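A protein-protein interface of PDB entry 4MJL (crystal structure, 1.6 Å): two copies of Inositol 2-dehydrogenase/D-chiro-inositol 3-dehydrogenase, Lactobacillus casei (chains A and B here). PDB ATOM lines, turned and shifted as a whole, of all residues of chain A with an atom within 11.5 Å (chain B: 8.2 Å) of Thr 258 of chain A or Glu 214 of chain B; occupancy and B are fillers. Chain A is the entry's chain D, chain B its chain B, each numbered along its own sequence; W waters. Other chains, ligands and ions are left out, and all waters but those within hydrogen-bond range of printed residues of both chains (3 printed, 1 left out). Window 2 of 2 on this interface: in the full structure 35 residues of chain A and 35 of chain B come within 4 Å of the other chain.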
ATOM      1  N   LYS A 151       1.966 -18.414  32.907  1.00  0.00           N
ATOM      2  CA  LYS A 151       0.565 -17.965  33.006  1.00  0.00           C
ATOM      3  C   LYS A 151      -0.286 -18.628  31.955  1.00  0.00           C
ATOM      4  O   LYS A 151      -1.428 -19.081  32.248  1.00  0.00           O
ATOM      5  CB  LYS A 151       0.511 -16.431  32.857  1.00  0.00           C
ATOM      6  CG  LYS A 151      -0.767 -15.743  33.317  1.00  0.00           C
ATOM      7  CD  LYS A 151      -0.968 -15.914  34.763  1.00  0.00           C
ATOM      8  CE  LYS A 151      -2.143 -14.989  35.181  1.00  0.00           C
ATOM      9  NZ  LYS A 151      -2.634 -15.372  36.587  1.00  0.00           N
ATOM     10  N   LEU A 152       0.227 -18.734  30.738  1.00  0.00           N
ATOM     11  CA  LEU A 152      -0.510 -19.414  29.674  1.00  0.00           C
ATOM     12  C   LEU A 152      -0.860 -20.846  30.102  1.00  0.00           C
ATOM     13  O   LEU A 152      -1.957 -21.341  29.829  1.00  0.00           O
ATOM     14  CB  LEU A 152       0.320 -19.461  28.384  1.00  0.00           C
ATOM     15  CG  LEU A 152      -0.187 -20.304  27.200  1.00  0.00           C
ATOM     16  CD1 LEU A 152      -1.475 -19.733  26.737  1.00  0.00           C
ATOM     17  CD2 LEU A 152       0.856 -20.283  26.085  1.00  0.00           C
ATOM     18  N   ASP A 153       0.108 -21.518  30.707  1.00  0.00           N
ATOM     19  CA  ASP A 153      -0.015 -22.950  31.042  1.00  0.00           C
ATOM     20  C   ASP A 153      -1.001 -23.233  32.200  1.00  0.00           C
ATOM     21  O   ASP A 153      -1.395 -24.373  32.426  1.00  0.00           O
ATOM     22  CB  ASP A 153       1.384 -23.530  31.326  1.00  0.00           C
ATOM     23  CG  ASP A 153       2.203 -23.705  30.031  1.00  0.00           C
ATOM     24  OD1 ASP A 153       1.593 -23.681  28.914  1.00  0.00           O
ATOM     25  OD2 ASP A 153       3.441 -23.921  30.122  1.00  0.00           O
ATOM     26  N   THR A 154      -1.411 -22.188  32.913  1.00  0.00           N
ATOM     27  CA  THR A 154      -2.458 -22.320  33.932  1.00  0.00           C
ATOM     28  C   THR A 154      -3.824 -22.522  33.303  1.00  0.00           C
ATOM     29  O   THR A 154      -4.740 -22.929  33.996  1.00  0.00           O
ATOM     30  CB  THR A 154      -2.554 -21.095  34.884  1.00  0.00           C
ATOM     31  OG1 THR A 154      -3.021 -19.943  34.159  1.00  0.00           O
ATOM     32  CG2 THR A 154      -1.199 -20.739  35.544  1.00  0.00           C
ATOM     33  N   GLY A 155      -3.978 -22.214  32.028  1.00  0.00           N
ATOM     34  CA  GLY A 155      -5.262 -22.313  31.342  1.00  0.00           C
ATOM     35  C   GLY A 155      -6.152 -21.084  31.487  1.00  0.00           C
ATOM     36  O   GLY A 155      -7.294 -21.084  31.025  1.00  0.00           O
ATOM     37  N   ILE A 156      -5.643 -20.034  32.107  1.00  0.00           N
ATOM     38  CA  ILE A 156      -6.430 -18.846  32.400  1.00  0.00           C
ATOM     39  C   ILE A 156      -7.022 -18.182  31.149  1.00  0.00           C
ATOM     40  O   ILE A 156      -8.079 -17.543  31.245  1.00  0.00           O
ATOM     41  CB  ILE A 156      -5.616 -17.837  33.299  1.00  0.00           C
ATOM     42  CG1 ILE A 156      -6.475 -16.644  33.764  1.00  0.00           C
ATOM     43  CG2 ILE A 156      -4.412 -17.290  32.575  1.00  0.00           C
ATOM     44  CD1 ILE A 156      -7.655 -16.990  34.436  1.00  0.00           C
ATOM     45  N   ILE A 157      -6.376 -18.327  29.991  1.00  0.00           N
ATOM     46  CA  ILE A 157      -6.909 -17.757  28.762  1.00  0.00           C
ATOM     47  C   ILE A 157      -7.401 -18.805  27.737  1.00  0.00           C
ATOM     48  O   ILE A 157      -7.716 -18.467  26.603  1.00  0.00           O
ATOM     49  CB  ILE A 157      -5.899 -16.736  28.066  1.00  0.00           C
ATOM     50  CG1 ILE A 157      -4.651 -17.441  27.539  1.00  0.00           C
ATOM     51  CG2 ILE A 157      -5.572 -15.544  28.999  1.00  0.00           C
ATOM     52  CD1 ILE A 157      -3.903 -16.558  26.509  1.00  0.00           C
ATOM     53  N   GLY A 158      -7.478 -20.070  28.153  1.00  0.00           N
ATOM     54  CA  GLY A 158      -7.930 -21.128  27.278  1.00  0.00           C
ATOM     55  C   GLY A 158      -6.802 -21.505  26.358  1.00  0.00           C
ATOM     56  O   GLY A 158      -5.640 -21.195  26.652  1.00  0.00           O
ATOM     57  N   ALA A 159      -7.118 -22.152  25.238  1.00  0.00           N
ATOM     58  CA  ALA A 159      -6.102 -22.621  24.285  1.00  0.00           C
ATOM     59  C   ALA A 159      -5.536 -21.439  23.514  1.00  0.00           C
ATOM     60  O   ALA A 159      -6.288 -20.505  23.171  1.00  0.00           O
ATOM     61  CB  ALA A 159      -6.711 -23.571  23.304  1.00  0.00           C
ATOM     62  N   PRO A 160      -4.231 -21.489  23.207  1.00  0.00           N
ATOM     63  CA  PRO A 160      -3.680 -20.452  22.333  1.00  0.00           C
ATOM     64  C   PRO A 160      -4.124 -20.607  20.858  1.00  0.00           C
ATOM     65  O   PRO A 160      -3.829 -21.646  20.238  1.00  0.00           O
ATOM     66  CB  PRO A 160      -2.145 -20.628  22.494  1.00  0.00           C
ATOM     67  CG  PRO A 160      -1.960 -22.113  22.830  1.00  0.00           C
ATOM     68  CD  PRO A 160      -3.221 -22.487  23.626  1.00  0.00           C
ATOM     69  N   LEU A 161      -4.787 -19.602  20.294  1.00  0.00           N
ATOM     70  CA  LEU A 161      -5.260 -19.665  18.921  1.00  0.00           C
ATOM     71  C   LEU A 161      -4.344 -18.958  17.932  1.00  0.00           C
ATOM     72  O   LEU A 161      -4.100 -19.427  16.807  1.00  0.00           O
ATOM     73  CB  LEU A 161      -6.639 -19.022  18.826  1.00  0.00           C
ATOM     74  CG  LEU A 161      -7.609 -19.510  19.899  1.00  0.00           C
ATOM     75  CD1 LEU A 161      -8.865 -18.592  19.936  1.00  0.00           C
ATOM     76  CD2 LEU A 161      -7.948 -20.945  19.599  1.00  0.00           C
ATOM     77  N   VAL A 162      -3.836 -17.798  18.358  1.00  0.00           N
ATOM     78  CA  VAL A 162      -2.973 -16.977  17.483  1.00  0.00           C
ATOM     79  C   VAL A 162      -1.879 -16.387  18.374  1.00  0.00           C
ATOM     80  O   VAL A 162      -2.129 -16.107  19.562  1.00  0.00           O
ATOM     81  CB  VAL A 162      -3.749 -15.833  16.807  1.00  0.00           C
ATOM     82  CG1 VAL A 162      -2.804 -14.939  16.012  1.00  0.00           C
ATOM     83  CG2 VAL A 162      -4.819 -16.410  15.821  1.00  0.00           C
ATOM     84  N   VAL A 254      -0.156 -13.455  23.134  1.00  0.00           N
ATOM     85  CA  VAL A 254      -0.815 -14.717  22.856  1.00  0.00           C
ATOM     86  C   VAL A 254      -2.342 -14.486  22.979  1.00  0.00           C
ATOM     87  O   VAL A 254      -2.832 -14.016  23.991  1.00  0.00           O
ATOM     88  CB  VAL A 254      -0.363 -15.834  23.838  1.00  0.00           C
ATOM     89  CG1 VAL A 254      -1.112 -17.127  23.523  1.00  0.00           C
ATOM     90  CG2 VAL A 254       1.154 -16.061  23.756  1.00  0.00           C
ATOM     91  N   ILE A 255      -3.054 -14.834  21.924  1.00  0.00           N
ATOM     92  CA  ILE A 255      -4.495 -14.658  21.857  1.00  0.00           C
ATOM     93  C   ILE A 255      -5.103 -16.042  22.200  1.00  0.00           C
ATOM     94  O   ILE A 255      -4.910 -17.006  21.449  1.00  0.00           O
ATOM     95  CB  ILE A 255      -4.915 -14.128  20.442  1.00  0.00           C
ATOM     96  CG1 ILE A 255      -4.368 -12.667  20.240  1.00  0.00           C
ATOM     97  CG2 ILE A 255      -6.455 -14.209  20.252  1.00  0.00           C
ATOM     98  CD1 ILE A 255      -3.283 -12.635  19.286  1.00  0.00           C
ATOM     99  N   GLY A 256      -5.819 -16.131  23.316  1.00  0.00           N
ATOM    100  CA  GLY A 256      -6.439 -17.395  23.724  1.00  0.00           C
ATOM    101  C   GLY A 256      -7.948 -17.348  23.504  1.00  0.00           C
ATOM    102  O   GLY A 256      -8.522 -16.317  23.138  1.00  0.00           O
ATOM    103  N   GLU A 257      -8.604 -18.459  23.791  1.00  0.00           N
ATOM    104  CA  GLU A 257     -10.041 -18.550  23.676  1.00  0.00           C
ATOM    105  C   GLU A 257     -10.790 -17.593  24.572  1.00  0.00           C
ATOM    106  O   GLU A 257     -11.849 -17.108  24.196  1.00  0.00           O
ATOM    107  CB  GLU A 257     -10.455 -19.994  23.979  1.00  0.00           C
ATOM    108  CG  GLU A 257      -9.985 -20.929  22.904  1.00  0.00           C
ATOM    109  CD  GLU A 257     -10.158 -22.426  23.297  1.00  0.00           C
ATOM    110  OE1 GLU A 257      -9.949 -22.779  24.471  1.00  0.00           O
ATOM    111  OE2 GLU A 257     -10.461 -23.206  22.380  1.00  0.00           O
ATOM    112  N   THR A 258     -10.269 -17.323  25.755  1.00  0.00           N
ATOM    113  CA  THR A 258     -11.019 -16.524  26.730  1.00  0.00           C
ATOM    114  C   THR A 258     -10.288 -15.302  27.231  1.00  0.00           C
ATOM    115  O   THR A 258     -10.784 -14.597  28.110  1.00  0.00           O
ATOM    116  CB  THR A 258     -11.471 -17.379  27.922  1.00  0.00           C
ATOM    117  OG1 THR A 258     -10.331 -17.749  28.683  1.00  0.00           O
ATOM    118  CG2 THR A 258     -12.160 -18.650  27.400  1.00  0.00           C
ATOM    119  N   GLY A 259      -9.122 -15.034  26.660  1.00  0.00           N
ATOM    120  CA  GLY A 259      -8.337 -13.898  27.110  1.00  0.00           C
ATOM    121  C   GLY A 259      -7.089 -13.745  26.291  1.00  0.00           C
ATOM    122  O   GLY A 259      -6.882 -14.493  25.340  1.00  0.00           O
ATOM    123  N   GLU A 260      -6.268 -12.757  26.648  1.00  0.00           N
ATOM    124  CA  GLU A 260      -4.973 -12.539  25.983  1.00  0.00           C
ATOM    125  C   GLU A 260      -3.898 -12.345  27.004  1.00  0.00           C
ATOM    126  O   GLU A 260      -4.173 -11.906  28.103  1.00  0.00           O
ATOM    127  CB  GLU A 260      -4.995 -11.308  25.073  1.00  0.00           C
ATOM    128  CG  GLU A 260      -6.039 -11.371  23.978  1.00  0.00           C
ATOM    129  CD  GLU A 260      -5.974 -10.202  23.021  1.00  0.00           C
ATOM    130  OE1 GLU A 260      -5.214  -9.246  23.308  1.00  0.00           O
ATOM    131  OE2 GLU A 260      -6.704 -10.205  21.981  1.00  0.00           O
ATOM    132  N   LEU A 261      -2.661 -12.716  26.654  1.00  0.00           N
ATOM    133  CA  LEU A 261      -1.481 -12.432  27.478  1.00  0.00           C
ATOM    134  C   LEU A 261      -0.441 -11.697  26.612  1.00  0.00           C
ATOM    135  O   LEU A 261      -0.231 -12.032  25.439  1.00  0.00           O
ATOM    136  CB  LEU A 261      -0.860 -13.734  27.987  1.00  0.00           C
ATOM    137  CG  LEU A 261      -1.600 -14.424  29.145  1.00  0.00           C
ATOM    138  CD1 LEU A 261      -1.173 -15.910  29.235  1.00  0.00           C
ATOM    139  CD2 LEU A 261      -1.384 -13.685  30.481  1.00  0.00           C
ATOM    140  N   GLN A 262       0.196 -10.683  27.192  1.00  0.00           N
ATOM    141  CA  GLN A 262       1.172  -9.868  26.469  1.00  0.00           C
ATOM    142  C   GLN A 262       2.374  -9.609  27.353  1.00  0.00           C
ATOM    143  O   GLN A 262       2.225  -9.356  28.565  1.00  0.00           O
ATOM    144  CB  GLN A 262       0.474  -8.543  26.150  1.00  0.00           C
ATOM    145  CG  GLN A 262       1.171  -7.625  25.333  1.00  0.00           C
ATOM    146  CD  GLN A 262       0.229  -6.534  24.944  1.00  0.00           C
ATOM    147  OE1 GLN A 262      -0.843  -6.821  24.371  1.00  0.00           O
ATOM    148  NE2 GLN A 262       0.584  -5.296  25.230  1.00  0.00           N
ATOM    149  N   PRO B 170     -16.568  -9.693  22.529  1.00  0.00           N
ATOM    150  CA  PRO B 170     -16.593 -10.738  23.569  1.00  0.00           C
ATOM    151  C   PRO B 170     -17.450 -11.965  23.187  1.00  0.00           C
ATOM    152  O   PRO B 170     -17.028 -13.069  23.455  1.00  0.00           O
ATOM    153  CB  PRO B 170     -17.213 -10.021  24.774  1.00  0.00           C
ATOM    154  CG  PRO B 170     -17.892  -8.836  24.232  1.00  0.00           C
ATOM    155  CD  PRO B 170     -17.180  -8.438  22.995  1.00  0.00           C
ATOM    156  N   ASN B 171     -18.600 -11.768  22.550  1.00  0.00           N
ATOM    157  CA  ASN B 171     -19.506 -12.891  22.208  1.00  0.00           C
ATOM    158  C   ASN B 171     -20.457 -12.387  21.116  1.00  0.00           C
ATOM    159  O   ASN B 171     -20.650 -11.176  20.958  1.00  0.00           O
ATOM    160  CB  ASN B 171     -20.285 -13.369  23.459  1.00  0.00           C
ATOM    161  CG  ASN B 171     -19.530 -14.502  24.305  1.00  0.00           C
ATOM    162  OD1 ASN B 171     -19.174 -15.589  23.764  1.00  0.00           O
ATOM    163  ND2 ASN B 171     -19.320 -14.240  25.645  1.00  0.00           N
ATOM    164  N   VAL B 172     -21.062 -13.306  20.353  1.00  0.00           N
ATOM    165  CA  VAL B 172     -21.995 -12.918  19.308  1.00  0.00           C
ATOM    166  C   VAL B 172     -23.360 -13.565  19.549  1.00  0.00           C
ATOM    167  O   VAL B 172     -23.472 -14.552  20.272  1.00  0.00           O
ATOM    168  CB  VAL B 172     -21.485 -13.246  17.896  1.00  0.00           C
ATOM    169  CG1 VAL B 172     -20.293 -12.367  17.577  1.00  0.00           C
ATOM    170  CG2 VAL B 172     -21.147 -14.744  17.741  1.00  0.00           C
ATOM    171  N   GLN B 211      -9.871 -23.477  15.588  1.00  0.00           N
ATOM    172  CA  GLN B 211     -11.216 -22.987  15.898  1.00  0.00           C
ATOM    173  C   GLN B 211     -11.343 -22.877  17.384  1.00  0.00           C
ATOM    174  O   GLN B 211     -10.943 -23.797  18.117  1.00  0.00           O
ATOM    175  CB  GLN B 211     -12.257 -23.968  15.294  1.00  0.00           C
ATOM    176  CG  GLN B 211     -13.715 -23.748  15.735  1.00  0.00           C
ATOM    177  CD  GLN B 211     -14.376 -22.659  14.982  1.00  0.00           C
ATOM    178  OE1 GLN B 211     -13.720 -21.898  14.253  1.00  0.00           O
ATOM    179  NE2 GLN B 211     -15.698 -22.538  15.140  1.00  0.00           N
ATOM    180  N   SER B 212     -11.881 -21.756  17.873  1.00  0.00           N
ATOM    181  CA  SER B 212     -12.130 -21.601  19.283  1.00  0.00           C
ATOM    182  C   SER B 212     -13.258 -22.482  19.820  1.00  0.00           C
ATOM    183  O   SER B 212     -14.334 -22.542  19.183  1.00  0.00           O
ATOM    184  CB  SER B 212     -12.505 -20.149  19.571  1.00  0.00           C
ATOM    185  OG  SER B 212     -12.749 -20.008  20.959  1.00  0.00           O
ATOM    186  N   ALA B 213     -13.010 -23.101  20.966  1.00  0.00           N
ATOM    187  CA  ALA B 213     -14.038 -23.877  21.703  1.00  0.00           C
ATOM    188  C   ALA B 213     -15.241 -22.990  22.087  1.00  0.00           C
ATOM    189  O   ALA B 213     -16.285 -23.507  22.494  1.00  0.00           O
ATOM    190  CB  ALA B 213     -13.483 -24.487  22.944  1.00  0.00           C
ATOM    191  N   GLU B 214     -15.092 -21.657  22.002  1.00  0.00           N
ATOM    192  CA  GLU B 214     -16.134 -20.765  22.499  1.00  0.00           C
ATOM    193  C   GLU B 214     -17.211 -20.523  21.441  1.00  0.00           C
ATOM    194  O   GLU B 214     -18.232 -19.906  21.743  1.00  0.00           O
ATOM    195  CB  GLU B 214     -15.570 -19.412  22.905  1.00  0.00           C
ATOM    196  CG  GLU B 214     -14.590 -19.407  24.052  1.00  0.00           C
ATOM    197  CD  GLU B 214     -15.202 -19.870  25.357  1.00  0.00           C
ATOM    198  OE1 GLU B 214     -14.492 -20.592  26.079  1.00  0.00           O
ATOM    199  OE2 GLU B 214     -16.399 -19.580  25.614  1.00  0.00           O
ATOM    200  N   VAL B 215     -16.994 -20.987  20.208  1.00  0.00           N
ATOM    201  CA  VAL B 215     -17.927 -20.725  19.145  1.00  0.00           C
ATOM    202  C   VAL B 215     -19.152 -21.606  19.344  1.00  0.00           C
ATOM    203  O   VAL B 215     -19.021 -22.814  19.602  1.00  0.00           O
ATOM    204  CB  VAL B 215     -17.312 -20.983  17.797  1.00  0.00           C
ATOM    205  CG1 VAL B 215     -18.351 -20.954  16.663  1.00  0.00           C
ATOM    206  CG2 VAL B 215     -16.208 -19.919  17.545  1.00  0.00           C
ATOM    207  N   ARG B 216     -20.355 -21.004  19.412  1.00  0.00           N
ATOM    208  CA  ARG B 216     -21.659 -21.645  19.514  1.00  0.00           C
ATOM    209  C   ARG B 216     -22.443 -21.500  18.217  1.00  0.00           C
ATOM    210  O   ARG B 216     -23.610 -21.923  18.153  1.00  0.00           O
ATOM    211  CB  ARG B 216     -22.400 -20.957  20.624  1.00  0.00           C
ATOM    212  CG  ARG B 216     -21.657 -21.112  21.828  1.00  0.00           C
ATOM    213  CD  ARG B 216     -21.661 -22.477  22.420  1.00  0.00           C
ATOM    214  NE  ARG B 216     -20.933 -22.581  23.667  1.00  0.00           N
ATOM    215  CZ  ARG B 216     -19.629 -22.925  23.723  1.00  0.00           C
ATOM    216  NH1 ARG B 216     -18.914 -23.119  22.594  1.00  0.00           N
ATOM    217  NH2 ARG B 216     -19.032 -23.033  24.884  1.00  0.00           N
ATOM    218  N   ASN B 217     -22.005 -20.903  17.176  1.00  0.00           N
ATOM    219  CA  ASN B 217     -22.783 -20.617  15.976  1.00  0.00           C
ATOM    220  C   ASN B 217     -22.404 -21.462  14.777  1.00  0.00           C
ATOM    221  O   ASN B 217     -21.228 -21.591  14.429  1.00  0.00           O
ATOM    222  CB  ASN B 217     -22.580 -19.166  15.517  1.00  0.00           C
ATOM    223  CG  ASN B 217     -23.195 -18.134  16.451  1.00  0.00           C
ATOM    224  OD1 ASN B 217     -23.218 -18.303  17.659  1.00  0.00           O
ATOM    225  ND2 ASN B 217     -23.696 -17.048  15.875  1.00  0.00           N
ATOM    226  N   LEU B 220     -19.816 -20.706  11.766  1.00  0.00           N
ATOM    227  CA  LEU B 220     -18.873 -19.608  12.153  1.00  0.00           C
ATOM    228  C   LEU B 220     -17.468 -20.122  12.440  1.00  0.00           C
ATOM    229  O   LEU B 220     -17.270 -20.935  13.327  1.00  0.00           O
ATOM    230  CB  LEU B 220     -19.377 -18.820  13.367  1.00  0.00           C
ATOM    231  CG  LEU B 220     -18.505 -17.659  13.916  1.00  0.00           C
ATOM    232  CD1 LEU B 220     -18.257 -16.545  12.909  1.00  0.00           C
ATOM    233  CD2 LEU B 220     -19.174 -17.059  15.144  1.00  0.00           C
ATOM    234  N   ASP B 222     -13.963 -18.860  14.005  1.00  0.00           N
ATOM    235  CA  ASP B 222     -13.469 -17.814  14.863  1.00  0.00           C
ATOM    236  C   ASP B 222     -12.273 -18.363  15.632  1.00  0.00           C
ATOM    237  O   ASP B 222     -12.350 -19.432  16.230  1.00  0.00           O
ATOM    238  CB  ASP B 222     -14.555 -17.348  15.843  1.00  0.00           C
ATOM    239  CG  ASP B 222     -14.173 -16.046  16.557  1.00  0.00           C
ATOM    240  OD1 ASP B 222     -13.815 -15.066  15.848  1.00  0.00           O
ATOM    241  OD2 ASP B 222     -14.215 -16.017  17.807  1.00  0.00           O
ATOM    242  N   HIS B 241     -11.705 -11.448  16.089  1.00  0.00           N
ATOM    243  CA  HIS B 241     -11.930 -12.446  17.119  1.00  0.00           C
ATOM    244  C   HIS B 241     -13.188 -12.052  17.855  1.00  0.00           C
ATOM    245  O   HIS B 241     -13.157 -11.144  18.707  1.00  0.00           O
ATOM    246  CB  HIS B 241     -10.708 -12.520  18.100  1.00  0.00           C
ATOM    247  CG  HIS B 241     -10.732 -13.686  19.042  1.00  0.00           C
ATOM    248  ND1 HIS B 241      -9.891 -13.788  20.120  1.00  0.00           N
ATOM    249  CD2 HIS B 241     -11.529 -14.784  19.084  1.00  0.00           C
ATOM    250  CE1 HIS B 241     -10.140 -14.913  20.770  1.00  0.00           C
ATOM    251  NE2 HIS B 241     -11.143 -15.529  20.162  1.00  0.00           N
ATOM    252  N   VAL B 242     -14.278 -12.782  17.573  1.00  0.00           N
ATOM    253  CA  VAL B 242     -15.598 -12.331  17.998  1.00  0.00           C
ATOM    254  C   VAL B 242     -16.199 -13.111  19.142  1.00  0.00           C
ATOM    255  O   VAL B 242     -17.241 -12.717  19.637  1.00  0.00           O
ATOM    256  CB  VAL B 242     -16.610 -12.208  16.827  1.00  0.00           C
ATOM    257  CG1 VAL B 242     -16.061 -11.212  15.775  1.00  0.00           C
ATOM    258  CG2 VAL B 242     -16.922 -13.577  16.222  1.00  0.00           C
ATOM    259  N   THR B 243     -15.516 -14.157  19.596  1.00  0.00           N
ATOM    260  CA  THR B 243     -15.919 -14.893  20.810  1.00  0.00           C
ATOM    261  C   THR B 243     -14.820 -14.793  21.861  1.00  0.00           C
ATOM    262  O   THR B 243     -14.589 -15.703  22.629  1.00  0.00           O
ATOM    263  CB  THR B 243     -16.295 -16.364  20.528  1.00  0.00           C
ATOM    264  OG1 THR B 243     -15.133 -17.104  20.100  1.00  0.00           O
ATOM    265  CG2 THR B 243     -17.330 -16.371  19.450  1.00  0.00           C
ATOM    266  N   ALA B 244     -14.141 -13.640  21.906  1.00  0.00           N
ATOM    267  CA  ALA B 244     -12.945 -13.463  22.737  1.00  0.00           C
ATOM    268  C   ALA B 244     -13.153 -13.467  24.243  1.00  0.00           C
ATOM    269  O   ALA B 244     -12.204 -13.563  24.994  1.00  0.00           O
ATOM    270  CB  ALA B 244     -12.268 -12.170  22.348  1.00  0.00           C
ATOM    271  N   GLN B 245     -14.404 -13.284  24.662  1.00  0.00           N
ATOM    272  CA  GLN B 245     -14.860 -13.304  26.056  1.00  0.00           C
ATOM    273  C   GLN B 245     -14.515 -12.072  26.886  1.00  0.00           C
ATOM    274  O   GLN B 245     -15.330 -11.565  27.632  1.00  0.00           O
ATOM    275  CB  GLN B 245     -14.404 -14.571  26.809  1.00  0.00           C
ATOM    276  CG  GLN B 245     -14.798 -15.897  26.125  1.00  0.00           C
ATOM    277  CD  GLN B 245     -16.298 -15.977  25.853  1.00  0.00           C
ATOM    278  OE1 GLN B 245     -17.116 -15.893  26.779  1.00  0.00           O
ATOM    279  NE2 GLN B 245     -16.659 -16.104  24.606  1.00  0.00           N
ATOM    280  N   TYR B 246     -13.285 -11.613  26.799  1.00  0.00           N
ATOM    281  CA  TYR B 246     -12.816 -10.698  27.835  1.00  0.00           C
ATOM    282  C   TYR B 246     -13.297  -9.261  27.671  1.00  0.00           C
ATOM    283  O   TYR B 246     -13.281  -8.513  28.618  1.00  0.00           O
ATOM    284  CB  TYR B 246     -11.280 -10.688  27.902  1.00  0.00           C
ATOM    285  CG  TYR B 246     -10.594  -9.871  26.818  1.00  0.00           C
ATOM    286  CD1 TYR B 246     -10.395  -8.490  26.971  1.00  0.00           C
ATOM    287  CD2 TYR B 246     -10.116 -10.477  25.671  1.00  0.00           C
ATOM    288  CE1 TYR B 246      -9.730  -7.767  25.978  1.00  0.00           C
ATOM    289  CE2 TYR B 246      -9.471  -9.764  24.676  1.00  0.00           C
ATOM    290  CZ  TYR B 246      -9.272  -8.424  24.833  1.00  0.00           C
ATOM    291  OH  TYR B 246      -8.629  -7.693  23.840  1.00  0.00           O
ATOM    292  N   GLY B 247     -13.635  -8.852  26.464  1.00  0.00           N
ATOM    293  CA  GLY B 247     -14.003  -7.478  26.258  1.00  0.00           C
ATOM    294  C   GLY B 247     -14.199  -7.155  24.810  1.00  0.00           C
ATOM    295  O   GLY B 247     -14.024  -8.016  23.959  1.00  0.00           O
HETATM  296  O   HOH W   1      -8.666 -11.955  21.807  1.00  0.00           O
HETATM  297  O   HOH W   2     -12.683 -17.481  21.553  1.00  0.00           O
HETATM  298  O   HOH W   3     -11.903 -22.196  26.657  1.00  0.00           O
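Printed residues of chain B within 4 Å of Gly 256 of chain A: His 241 (3.2 Å). Printed residues of chain B within 4 Å of Glu 257 of chain A: Ser 212 (3.5 Å), Ala 213 (2.9 Å), Glu 214 (3.6 Å), Thr 243 (3.5 Å), Ala 244 (3.7 Å) and Gln 245 (3.7 Å). Of the printed residues of chain A, Ser 212 of chain B touches Leu 161 (3.98 Å) and Glu 257 (3.5 Å). Of chain A, only Glu 257 and Thr 258 come within 4 Å of Glu 214 of chain B. No residue of chain A comes within 4 Å of Val 215 of chain B. No residue of chain A comes within 4 Å of Arg 216 of chain B. Printed residues of chain A within 4 Å of His 241 of chain B: Leu 161, Ile 255 and Gly 256. Of chain A, only Glu 257 comes within 4 Å of Thr 243 of chain B. Gln 245 of chain B touches two residues of chain A. Of the printed residues of chain A, Tyr 246 of chain B touches Thr 258 and Glu 260. The nearest residue of chain B that does not touch Thr 258 of chain A is Thr 243 of chain B (5.5 Å). The nearest residue of chain A that does not touch Glu 214 of chain B is Gly 158 of chain A (6.7 Å).
NE2 of His 241 of chain B touches CD1 of Leu 161 of chain A, at 3.8 Å. ND1 of His 241 of chain B touches CG2 of Ile 255 of chain A (3.5 Å). OG of Ser 212 of chain B touches CG of Glu 257 of chain A, at 3.5 Å. Glu 257 of chain A touches Glu 214 of chain B. Glu 257 of chain A touches Ala 244 of chain B (O to O, 3.7 Å). O of Glu 257 of chain A touches CG of Gln 245 of chain B (3.7 Å). O of Ala 244 of chain B touches C of Thr 258 of chain A (3.4 Å). Tyr 246 of chain B touches Thr 258 of chain A. N of Gly 259 of chain A touches O of Ala 244 of chain B, at 3.8 Å. Glu 260 of chain A touches Tyr 246 of chain B (OE2 to OH, 3.7 Å).
No position is printed for both chains. Of the 16 pairs that touch across the chains among the printed residues, none has its exchanged pair printed and touching as well.
Of the 19 printed residues of chain B, 8 touch a printed residue of chain A. Printed residues of chain B that touch a printed residue of chain A: Ser 212, Ala 213, Glu 214, His 241, Thr 243, Ala 244, Gln 245 and Tyr 246. Hydrophobic or aromatic side chains of chain B that line the printed part of chain A: Ala 213, His 241 and Tyr 246. Of the 21 printed residues of chain A, 7 touch a printed residue of chain B. Printed residues of chain A that touch a printed residue of chain B: Leu 161, Ile 255, Gly 256, Glu 257, Thr 258, Gly 259 and Glu 260. Among the printed residues, 16 pairs touch across the chains.
The backbone carbonyl oxygen (O) of Glu 257 of chain A lies close to the backbone carbonyl oxygen (O) of Thr 243 of chain B. The side-chain carboxylate (OE2) of Glu 257 of chain A lies within hydrogen-bond range of the backbone NH (N) of Ala 213 of chain B (2.9 Å).
Water W2 lies within hydrogen-bond range of OG of Ser 212 of chain B (2.6 Å), O of Glu 257 of chain A (2.8 Å), O of Thr 243 of chain B (2.8 Å) and NE2 of His 241 of chain B (2.8 Å). Water W1 lies within hydrogen-bond range of the side-chain carboxylate of Glu 260 of chain A and a ring nitrogen (ND1) of His 241 of chain B. Water W3 lies within hydrogen-bond range of the side-chain carboxylate (OE1) of Glu 257 of chain A (3.0 Å) and the side-chain carboxylate (OE1) of Glu 214 of chain B (3.1 Å).
The side-chain carboxylate (OD2) of Asp 222 of chain B sits at hydrogen-bond distance from the side-chain hydroxyl (OG1) of Thr 243 of chain B (2.7 Å). The backbone carbonyl oxygen (O) of Pro 170 of chain B is in hydrogen-bond range of the backbone NH (N) of Ala 244 of chain B, 3.3 Å away. OE1 of Glu 257 of chain A sits at hydrogen-bond distance from N of Ala 159 of chain A, 3.0 Å away. NE2 of Gln 245 of chain B sits at hydrogen-bond distance from OD1 of Asn 171 of chain B (2.7 Å).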
